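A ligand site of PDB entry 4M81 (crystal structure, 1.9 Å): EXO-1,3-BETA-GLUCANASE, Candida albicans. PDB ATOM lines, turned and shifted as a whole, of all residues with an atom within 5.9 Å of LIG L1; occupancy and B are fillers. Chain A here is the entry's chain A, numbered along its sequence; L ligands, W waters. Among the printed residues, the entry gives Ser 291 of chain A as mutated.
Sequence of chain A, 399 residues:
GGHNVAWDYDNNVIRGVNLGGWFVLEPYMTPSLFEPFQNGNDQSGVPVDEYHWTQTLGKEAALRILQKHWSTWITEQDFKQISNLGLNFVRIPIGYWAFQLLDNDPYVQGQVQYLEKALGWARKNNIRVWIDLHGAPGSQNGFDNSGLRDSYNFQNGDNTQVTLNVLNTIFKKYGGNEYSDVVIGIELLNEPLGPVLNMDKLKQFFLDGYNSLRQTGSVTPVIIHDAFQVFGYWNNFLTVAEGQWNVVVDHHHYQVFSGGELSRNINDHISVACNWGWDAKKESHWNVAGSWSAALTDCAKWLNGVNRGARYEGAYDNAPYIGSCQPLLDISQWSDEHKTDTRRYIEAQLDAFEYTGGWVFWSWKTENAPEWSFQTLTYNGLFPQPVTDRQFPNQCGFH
An oxygen (O5) of LIG L1 lies within hydrogen-bond range of an oxygen (O6) of LG2 L2 (2.5 Å).
The side-chain hydroxyl of Tyr 254 lies within hydrogen-bond range of an oxygen (O4) of LIG L1 (3.2 Å).
The side-chain amide nitrogen (ND2) of Asn 145 is in hydrogen-bond range of an oxygen (O4) of LG2 L2, at 3.2 Å.
The side-chain amide nitrogen (ND2) of Asn 145 sits close to an oxygen (O2) of LIG L1.
An oxygen (O2) of LIG L1 lies within hydrogen-bond range of a ring nitrogen (NE2) of His 134, at 2.9 Å.
The indole nitrogen (NE1) of Trp 362 sits at hydrogen-bond distance from an oxygen (O3) of LIG L1, 3.1 Å away.
ND2 of Asn 190 is in hydrogen-bond range of O1 of LIG L1.
The side-chain carboxylate of Glu 26 lies within hydrogen-bond range of an oxygen (O3) of LIG L1, at 2.5 Å.
An oxygen (O3) of LIG L1 is in hydrogen-bond range of the side-chain hydroxyl (OH) of Tyr 28.
NE1 of Trp 362 lies within hydrogen-bond range of SD of Met 29 (3.3 Å).
The backbone NH (N) of Trp 362 is in hydrogen-bond range of the backbone carbonyl oxygen (O) of Trp 292 (2.7 Å).
The indole nitrogen (NE1) of Trp 362 sits at hydrogen-bond distance from the side-chain hydroxyl (OH) of Tyr 28 (2.8 Å).
The side-chain amide oxygen (OD1) of Asn 190 lies within hydrogen-bond range of the guanidinium group (NH2) of Arg 91.
The guanidinium group of Arg 91 lies within hydrogen-bond range of the side-chain hydroxyl of Ser 291.
The side-chain amide nitrogen of Asn 190 lies close to a ring nitrogen (NE2) of His 134 (3.3 Å).
OE2 of Glu 191 is in hydrogen-bond range of ND1 of His 252 (2.5 Å).
Water W1 lies within hydrogen-bond range of O5 of LIG L1 (2.6 Å), O of Leu 303 (2.7 Å) and O4 of LG2 L2 (3.0 Å).
Water W2 lies within hydrogen-bond range of OG of Ser 291 (2.6 Å), O1 of LIG L1 (2.7 Å), NH1 of Arg 91 (2.9 Å) and OD1 of Asn 190 (3.2 Å).
The side-chain hydroxyl of Ser 291 sits close to a fluorine (F1) of LIG L1 (3.3 Å).
Residues that only touch LIG L1: Phe 257, Glu 191 and Trp 372.
Hydrophobic or aromatic side chains within 4 Å of LIG L1: Tyr 28, His 134, Tyr 254, Phe 257, Trp 362 and Trp 372.
Within 4 Å of LIG L1: Glu 26, Tyr 28, His 134, Asn 145, Asn 190, Glu 191, Tyr 254, Phe 257, Ser 291, Trp 362 and Trp 372.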
ATOM      1  N   GLU A  26     -26.464 -11.214  23.902  1.00  0.00           N
ATOM      2  CA  GLU A  26     -25.629 -12.403  24.046  1.00  0.00           C
ATOM      3  C   GLU A  26     -24.339 -12.129  23.327  1.00  0.00           C
ATOM      4  O   GLU A  26     -24.332 -11.949  22.103  1.00  0.00           O
ATOM      5  CB  GLU A  26     -26.317 -13.627  23.445  1.00  0.00           C
ATOM      6  CG  GLU A  26     -27.714 -13.818  23.987  1.00  0.00           C
ATOM      7  CD  GLU A  26     -28.209 -15.242  23.901  1.00  0.00           C
ATOM      8  OE1 GLU A  26     -27.380 -16.173  23.787  1.00  0.00           O
ATOM      9  OE2 GLU A  26     -29.440 -15.413  23.951  1.00  0.00           O
ATOM     10  N   TYR A  28     -21.853 -13.817  22.236  1.00  0.00           N
ATOM     11  CA  TYR A  28     -21.473 -14.591  21.053  1.00  0.00           C
ATOM     12  C   TYR A  28     -22.301 -14.222  19.824  1.00  0.00           C
ATOM     13  O   TYR A  28     -21.849 -14.426  18.690  1.00  0.00           O
ATOM     14  CB  TYR A  28     -21.508 -16.102  21.301  1.00  0.00           C
ATOM     15  CG  TYR A  28     -22.859 -16.762  21.087  1.00  0.00           C
ATOM     16  CD1 TYR A  28     -23.805 -16.807  22.111  1.00  0.00           C
ATOM     17  CD2 TYR A  28     -23.159 -17.378  19.868  1.00  0.00           C
ATOM     18  CE1 TYR A  28     -25.045 -17.447  21.906  1.00  0.00           C
ATOM     19  CE2 TYR A  28     -24.382 -18.006  19.669  1.00  0.00           C
ATOM     20  CZ  TYR A  28     -25.327 -18.038  20.682  1.00  0.00           C
ATOM     21  OH  TYR A  28     -26.544 -18.663  20.453  1.00  0.00           O
ATOM     22  N   MET A  29     -23.484 -13.667  20.039  1.00  0.00           N
ATOM     23  CA  MET A  29     -24.386 -13.314  18.943  1.00  0.00           C
ATOM     24  C   MET A  29     -24.122 -11.895  18.428  1.00  0.00           C
ATOM     25  O   MET A  29     -24.153 -11.652  17.223  1.00  0.00           O
ATOM     26  CB  MET A  29     -25.849 -13.455  19.379  1.00  0.00           C
ATOM     27  CG  MET A  29     -26.178 -14.846  19.925  1.00  0.00           C
ATOM     28  SD  MET A  29     -27.923 -15.044  20.292  1.00  0.00           S
ATOM     29  CE  MET A  29     -28.604 -14.960  18.619  1.00  0.00           C
ATOM     30  N   ARG A  91     -39.992 -17.529  17.944  1.00  0.00           N
ATOM     31  CA  ARG A  91     -39.955 -17.482  19.400  1.00  0.00           C
ATOM     32  C   ARG A  91     -39.217 -16.202  19.749  1.00  0.00           C
ATOM     33  O   ARG A  91     -38.152 -15.951  19.212  1.00  0.00           O
ATOM     34  CB  ARG A  91     -39.174 -18.690  19.936  1.00  0.00           C
ATOM     35  CG  ARG A  91     -39.080 -18.773  21.447  1.00  0.00           C
ATOM     36  CD  ARG A  91     -38.578 -20.168  21.773  1.00  0.00           C
ATOM     37  NE  ARG A  91     -38.337 -20.404  23.185  1.00  0.00           N
ATOM     38  CZ  ARG A  91     -37.151 -20.292  23.762  1.00  0.00           C
ATOM     39  NH1 ARG A  91     -36.097 -19.917  23.036  1.00  0.00           N
ATOM     40  NH2 ARG A  91     -37.015 -20.545  25.045  1.00  0.00           N
ATOM     41  N   HIS A 134     -37.037 -15.052  28.905  1.00  0.00           N
ATOM     42  CA  HIS A 134     -35.709 -15.641  28.790  1.00  0.00           C
ATOM     43  C   HIS A 134     -34.829 -15.420  30.011  1.00  0.00           C
ATOM     44  O   HIS A 134     -33.833 -16.131  30.204  1.00  0.00           O
ATOM     45  CB  HIS A 134     -35.021 -15.097  27.543  1.00  0.00           C
ATOM     46  CG  HIS A 134     -34.140 -16.082  26.852  1.00  0.00           C
ATOM     47  ND1 HIS A 134     -34.649 -17.127  26.107  1.00  0.00           N
ATOM     48  CD2 HIS A 134     -32.793 -16.199  26.794  1.00  0.00           C
ATOM     49  CE1 HIS A 134     -33.647 -17.843  25.627  1.00  0.00           C
ATOM     50  NE2 HIS A 134     -32.514 -17.302  26.026  1.00  0.00           N
ATOM     51  N   PHE A 143     -26.528 -18.493  33.224  1.00  0.00           N
ATOM     52  CA  PHE A 143     -26.024 -18.346  31.850  1.00  0.00           C
ATOM     53  C   PHE A 143     -26.036 -16.866  31.515  1.00  0.00           C
ATOM     54  O   PHE A 143     -26.889 -16.125  31.989  1.00  0.00           O
ATOM     55  CB  PHE A 143     -26.939 -19.047  30.837  1.00  0.00           C
ATOM     56  CG  PHE A 143     -27.193 -20.515  31.103  1.00  0.00           C
ATOM     57  CD1 PHE A 143     -26.294 -21.286  31.807  1.00  0.00           C
ATOM     58  CD2 PHE A 143     -28.350 -21.121  30.610  1.00  0.00           C
ATOM     59  CE1 PHE A 143     -26.551 -22.644  32.036  1.00  0.00           C
ATOM     60  CE2 PHE A 143     -28.597 -22.458  30.820  1.00  0.00           C
ATOM     61  CZ  PHE A 143     -27.697 -23.220  31.533  1.00  0.00           C
ATOM     62  N   ASN A 145     -27.084 -15.564  28.939  1.00  0.00           N
ATOM     63  CA  ASN A 145     -28.327 -15.296  28.232  1.00  0.00           C
ATOM     64  C   ASN A 145     -29.545 -15.146  29.141  1.00  0.00           C
ATOM     65  O   ASN A 145     -30.641 -14.884  28.646  1.00  0.00           O
ATOM     66  CB  ASN A 145     -28.574 -16.359  27.148  1.00  0.00           C
ATOM     67  CG  ASN A 145     -28.621 -17.751  27.703  1.00  0.00           C
ATOM     68  OD1 ASN A 145     -29.523 -18.085  28.457  1.00  0.00           O
ATOM     69  ND2 ASN A 145     -27.636 -18.577  27.340  1.00  0.00           N
ATOM     70  N   ASN A 190     -37.503 -19.468  30.353  1.00  0.00           N
ATOM     71  CA  ASN A 190     -36.503 -20.169  29.555  1.00  0.00           C
ATOM     72  C   ASN A 190     -35.477 -20.863  30.437  1.00  0.00           C
ATOM     73  O   ASN A 190     -34.940 -20.247  31.359  1.00  0.00           O
ATOM     74  CB  ASN A 190     -35.765 -19.211  28.635  1.00  0.00           C
ATOM     75  CG  ASN A 190     -34.639 -19.895  27.887  1.00  0.00           C
ATOM     76  OD1 ASN A 190     -34.909 -20.753  27.038  1.00  0.00           O
ATOM     77  ND2 ASN A 190     -33.385 -19.565  28.214  1.00  0.00           N
ATOM     78  N   GLU A 191     -35.210 -22.133  30.145  1.00  0.00           N
ATOM     79  CA  GLU A 191     -34.081 -22.852  30.756  1.00  0.00           C
ATOM     80  C   GLU A 191     -33.802 -22.652  32.249  1.00  0.00           C
ATOM     81  O   GLU A 191     -32.690 -22.313  32.628  1.00  0.00           O
ATOM     82  CB  GLU A 191     -32.792 -22.598  29.949  1.00  0.00           C
ATOM     83  CG  GLU A 191     -32.930 -23.060  28.500  1.00  0.00           C
ATOM     84  CD  GLU A 191     -31.605 -23.141  27.750  1.00  0.00           C
ATOM     85  OE1 GLU A 191     -30.615 -22.544  28.206  1.00  0.00           O
ATOM     86  OE2 GLU A 191     -31.573 -23.808  26.694  1.00  0.00           O
ATOM     87  N   HIS A 252     -34.907 -28.262  24.607  1.00  0.00           N
ATOM     88  CA  HIS A 252     -33.755 -27.709  23.876  1.00  0.00           C
ATOM     89  C   HIS A 252     -32.734 -28.825  23.644  1.00  0.00           C
ATOM     90  O   HIS A 252     -32.578 -29.714  24.468  1.00  0.00           O
ATOM     91  CB  HIS A 252     -33.148 -26.535  24.634  1.00  0.00           C
ATOM     92  CG  HIS A 252     -34.082 -25.370  24.769  1.00  0.00           C
ATOM     93  ND1 HIS A 252     -33.767 -24.242  25.486  1.00  0.00           N
ATOM     94  CD2 HIS A 252     -35.330 -25.177  24.283  1.00  0.00           C
ATOM     95  CE1 HIS A 252     -34.776 -23.384  25.427  1.00  0.00           C
ATOM     96  NE2 HIS A 252     -35.737 -23.933  24.699  1.00  0.00           N
ATOM     97  N   TYR A 254     -28.779 -29.667  22.106  1.00  0.00           N
ATOM     98  CA  TYR A 254     -27.464 -29.373  21.544  1.00  0.00           C
ATOM     99  C   TYR A 254     -26.536 -30.540  21.823  1.00  0.00           C
ATOM    100  O   TYR A 254     -26.808 -31.340  22.713  1.00  0.00           O
ATOM    101  CB  TYR A 254     -26.867 -28.130  22.187  1.00  0.00           C
ATOM    102  CG  TYR A 254     -27.670 -26.888  21.952  1.00  0.00           C
ATOM    103  CD1 TYR A 254     -27.701 -26.307  20.697  1.00  0.00           C
ATOM    104  CD2 TYR A 254     -28.391 -26.300  22.983  1.00  0.00           C
ATOM    105  CE1 TYR A 254     -28.429 -25.163  20.476  1.00  0.00           C
ATOM    106  CE2 TYR A 254     -29.126 -25.141  22.769  1.00  0.00           C
ATOM    107  CZ  TYR A 254     -29.137 -24.581  21.504  1.00  0.00           C
ATOM    108  OH  TYR A 254     -29.855 -23.426  21.254  1.00  0.00           O
ATOM    109  N   PHE A 257     -22.007 -28.873  24.411  1.00  0.00           N
ATOM    110  CA  PHE A 257     -21.688 -28.231  25.693  1.00  0.00           C
ATOM    111  C   PHE A 257     -20.991 -29.128  26.725  1.00  0.00           C
ATOM    112  O   PHE A 257     -21.011 -28.841  27.922  1.00  0.00           O
ATOM    113  CB  PHE A 257     -22.896 -27.491  26.280  1.00  0.00           C
ATOM    114  CG  PHE A 257     -23.281 -26.279  25.471  1.00  0.00           C
ATOM    115  CD1 PHE A 257     -22.459 -25.156  25.441  1.00  0.00           C
ATOM    116  CD2 PHE A 257     -24.454 -26.270  24.728  1.00  0.00           C
ATOM    117  CE1 PHE A 257     -22.800 -24.033  24.687  1.00  0.00           C
ATOM    118  CE2 PHE A 257     -24.807 -25.150  23.969  1.00  0.00           C
ATOM    119  CZ  PHE A 257     -23.978 -24.032  23.944  1.00  0.00           C
ATOM    120  N   SER A 291     -35.258 -24.734  20.852  1.00  0.00           N
ATOM    121  CA  SER A 291     -33.902 -24.266  20.584  1.00  0.00           C
ATOM    122  C   SER A 291     -33.005 -25.424  20.226  1.00  0.00           C
ATOM    123  O   SER A 291     -33.019 -26.462  20.892  1.00  0.00           O
ATOM    124  CB  SER A 291     -33.304 -23.503  21.757  1.00  0.00           C
ATOM    125  OG  SER A 291     -33.903 -22.231  21.903  1.00  0.00           O
ATOM    126  N   TRP A 292     -32.216 -25.235  19.173  1.00  0.00           N
ATOM    127  CA  TRP A 292     -31.283 -26.219  18.667  1.00  0.00           C
ATOM    128  C   TRP A 292     -30.509 -25.453  17.618  1.00  0.00           C
ATOM    129  O   TRP A 292     -30.908 -24.354  17.232  1.00  0.00           O
ATOM    130  CB  TRP A 292     -32.010 -27.390  18.006  1.00  0.00           C
ATOM    131  CG  TRP A 292     -32.867 -26.999  16.805  1.00  0.00           C
ATOM    132  CD1 TRP A 292     -34.094 -26.384  16.844  1.00  0.00           C
ATOM    133  CD2 TRP A 292     -32.592 -27.242  15.417  1.00  0.00           C
ATOM    134  NE1 TRP A 292     -34.576 -26.201  15.564  1.00  0.00           N
ATOM    135  CE2 TRP A 292     -33.678 -26.731  14.671  1.00  0.00           C
ATOM    136  CE3 TRP A 292     -31.526 -27.836  14.730  1.00  0.00           C
ATOM    137  CZ2 TRP A 292     -33.731 -26.790  13.276  1.00  0.00           C
ATOM    138  CZ3 TRP A 292     -31.578 -27.885  13.345  1.00  0.00           C
ATOM    139  CH2 TRP A 292     -32.683 -27.370  12.635  1.00  0.00           C
ATOM    140  N   LEU A 303     -19.219 -18.261  22.903  1.00  0.00           N
ATOM    141  CA  LEU A 303     -20.417 -19.091  23.057  1.00  0.00           C
ATOM    142  C   LEU A 303     -20.598 -19.546  24.517  1.00  0.00           C
ATOM    143  O   LEU A 303     -21.706 -19.579  25.042  1.00  0.00           O
ATOM    144  CB  LEU A 303     -20.354 -20.308  22.137  1.00  0.00           C
ATOM    145  CG  LEU A 303     -21.536 -21.270  22.280  1.00  0.00           C
ATOM    146  CD1 LEU A 303     -22.826 -20.638  21.744  1.00  0.00           C
ATOM    147  CD2 LEU A 303     -21.267 -22.595  21.590  1.00  0.00           C
ATOM    148  N   TRP A 362     -32.158 -21.942  16.837  1.00  0.00           N
ATOM    149  CA  TRP A 362     -31.430 -20.835  17.472  1.00  0.00           C
ATOM    150  C   TRP A 362     -30.141 -20.552  16.695  1.00  0.00           C
ATOM    151  O   TRP A 362     -29.206 -21.340  16.776  1.00  0.00           O
ATOM    152  CB  TRP A 362     -31.084 -21.124  18.943  1.00  0.00           C
ATOM    153  CG  TRP A 362     -30.585 -19.856  19.602  1.00  0.00           C
ATOM    154  CD1 TRP A 362     -29.382 -19.247  19.386  1.00  0.00           C
ATOM    155  CD2 TRP A 362     -31.298 -19.013  20.506  1.00  0.00           C
ATOM    156  NE1 TRP A 362     -29.298 -18.088  20.106  1.00  0.00           N
ATOM    157  CE2 TRP A 362     -30.459 -17.915  20.805  1.00  0.00           C
ATOM    158  CE3 TRP A 362     -32.561 -19.092  21.115  1.00  0.00           C
ATOM    159  CZ2 TRP A 362     -30.844 -16.899  21.686  1.00  0.00           C
ATOM    160  CZ3 TRP A 362     -32.940 -18.075  21.966  1.00  0.00           C
ATOM    161  CH2 TRP A 362     -32.081 -16.996  22.254  1.00  0.00           C
ATOM    162  N   TRP A 372     -24.808 -20.816  14.155  1.00  0.00           N
ATOM    163  CA  TRP A 372     -25.911 -20.339  14.983  1.00  0.00           C
ATOM    164  C   TRP A 372     -26.827 -19.369  14.226  1.00  0.00           C
ATOM    165  O   TRP A 372     -27.624 -18.666  14.833  1.00  0.00           O
ATOM    166  CB  TRP A 372     -25.327 -19.682  16.229  1.00  0.00           C
ATOM    167  CG  TRP A 372     -24.534 -20.656  17.059  1.00  0.00           C
ATOM    168  CD1 TRP A 372     -23.191 -20.908  17.003  1.00  0.00           C
ATOM    169  CD2 TRP A 372     -25.066 -21.528  18.052  1.00  0.00           C
ATOM    170  NE1 TRP A 372     -22.853 -21.873  17.929  1.00  0.00           N
ATOM    171  CE2 TRP A 372     -23.988 -22.276  18.584  1.00  0.00           C
ATOM    172  CE3 TRP A 372     -26.341 -21.757  18.570  1.00  0.00           C
ATOM    173  CZ2 TRP A 372     -24.169 -23.231  19.583  1.00  0.00           C
ATOM    174  CZ3 TRP A 372     -26.505 -22.696  19.554  1.00  0.00           C
ATOM    175  CH2 TRP A 372     -25.424 -23.419  20.062  1.00  0.00           C
HETATM  176  C1  LIG L   1     -30.139 -21.772  24.356  1.00  0.00           C
HETATM  177  C2  LIG L   1     -30.211 -20.447  25.113  1.00  0.00           C
HETATM  178  C3  LIG L   1     -29.856 -19.296  24.179  1.00  0.00           C
HETATM  179  C4  LIG L   1     -28.434 -19.551  23.712  1.00  0.00           C
HETATM  180  C5  LIG L   1     -28.361 -20.920  23.017  1.00  0.00           C
HETATM  181  C6  LIG L   1     -26.928 -21.317  22.696  1.00  0.00           C
HETATM  182  F1  LIG L   1     -30.972 -21.729  23.264  1.00  0.00           F
HETATM  183  O1  LIG L   1     -31.530 -20.248  25.593  1.00  0.00           O
HETATM  184  O2  LIG L   1     -29.986 -18.044  24.869  1.00  0.00           O
HETATM  185  O3  LIG L   1     -27.955 -18.481  22.884  1.00  0.00           O
HETATM  186  O4  LIG L   1     -28.815 -21.942  23.897  1.00  0.00           O
HETATM  187  O5  LIG L   1     -26.226 -21.483  23.928  1.00  0.00           O
HETATM  188  C1  LG2 L   2     -25.465 -24.810  28.859  1.00  0.00           C
HETATM  189  N1  LG2 L   2     -27.668 -29.509  32.650  1.00  0.00           N
HETATM  190  O1  LG2 L   2     -25.221 -26.212  28.920  1.00  0.00           O
HETATM  191  C2  LG2 L   2     -24.132 -24.118  28.621  1.00  0.00           C
HETATM  192  O2  LG2 L   2     -23.282 -24.347  29.755  1.00  0.00           O
HETATM  193  C3  LG2 L   2     -24.330 -22.617  28.425  1.00  0.00           C
HETATM  194  O3  LG2 L   2     -23.106 -21.967  28.080  1.00  0.00           O
HETATM  195  C4  LG2 L   2     -25.317 -22.396  27.291  1.00  0.00           C
HETATM  196  O4  LG2 L   2     -25.580 -20.991  27.197  1.00  0.00           O
HETATM  197  C5  LG2 L   2     -26.600 -23.149  27.607  1.00  0.00           C
HETATM  198  O5  LG2 L   2     -26.337 -24.553  27.768  1.00  0.00           O
HETATM  199  C6  LG2 L   2     -27.587 -22.986  26.479  1.00  0.00           C
HETATM  200  O6  LG2 L   2     -27.008 -23.448  25.259  1.00  0.00           O
HETATM  201  C7  LG2 L   2     -25.858 -27.006  29.839  1.00  0.00           C
HETATM  202  O7  LG2 L   2     -27.089 -30.516  33.003  1.00  0.00           O
HETATM  203  C8  LG2 L   2     -25.208 -28.155  30.279  1.00  0.00           C
HETATM  204  O8  LG2 L   2     -28.764 -29.252  33.101  1.00  0.00           O
HETATM  205  C9  LG2 L   2     -25.815 -28.978  31.205  1.00  0.00           C
HETATM  206  C10 LG2 L   2     -27.070 -28.656  31.704  1.00  0.00           C
HETATM  207  C11 LG2 L   2     -27.720 -27.498  31.274  1.00  0.00           C
HETATM  208  C12 LG2 L   2     -27.104 -26.667  30.340  1.00  0.00           C
HETATM  209  O   HOH W   1     -24.417 -19.799  24.752  1.00  0.00           O
HETATM  210  O   HOH W   2     -33.641 -20.898  24.102  1.00  0.00           O
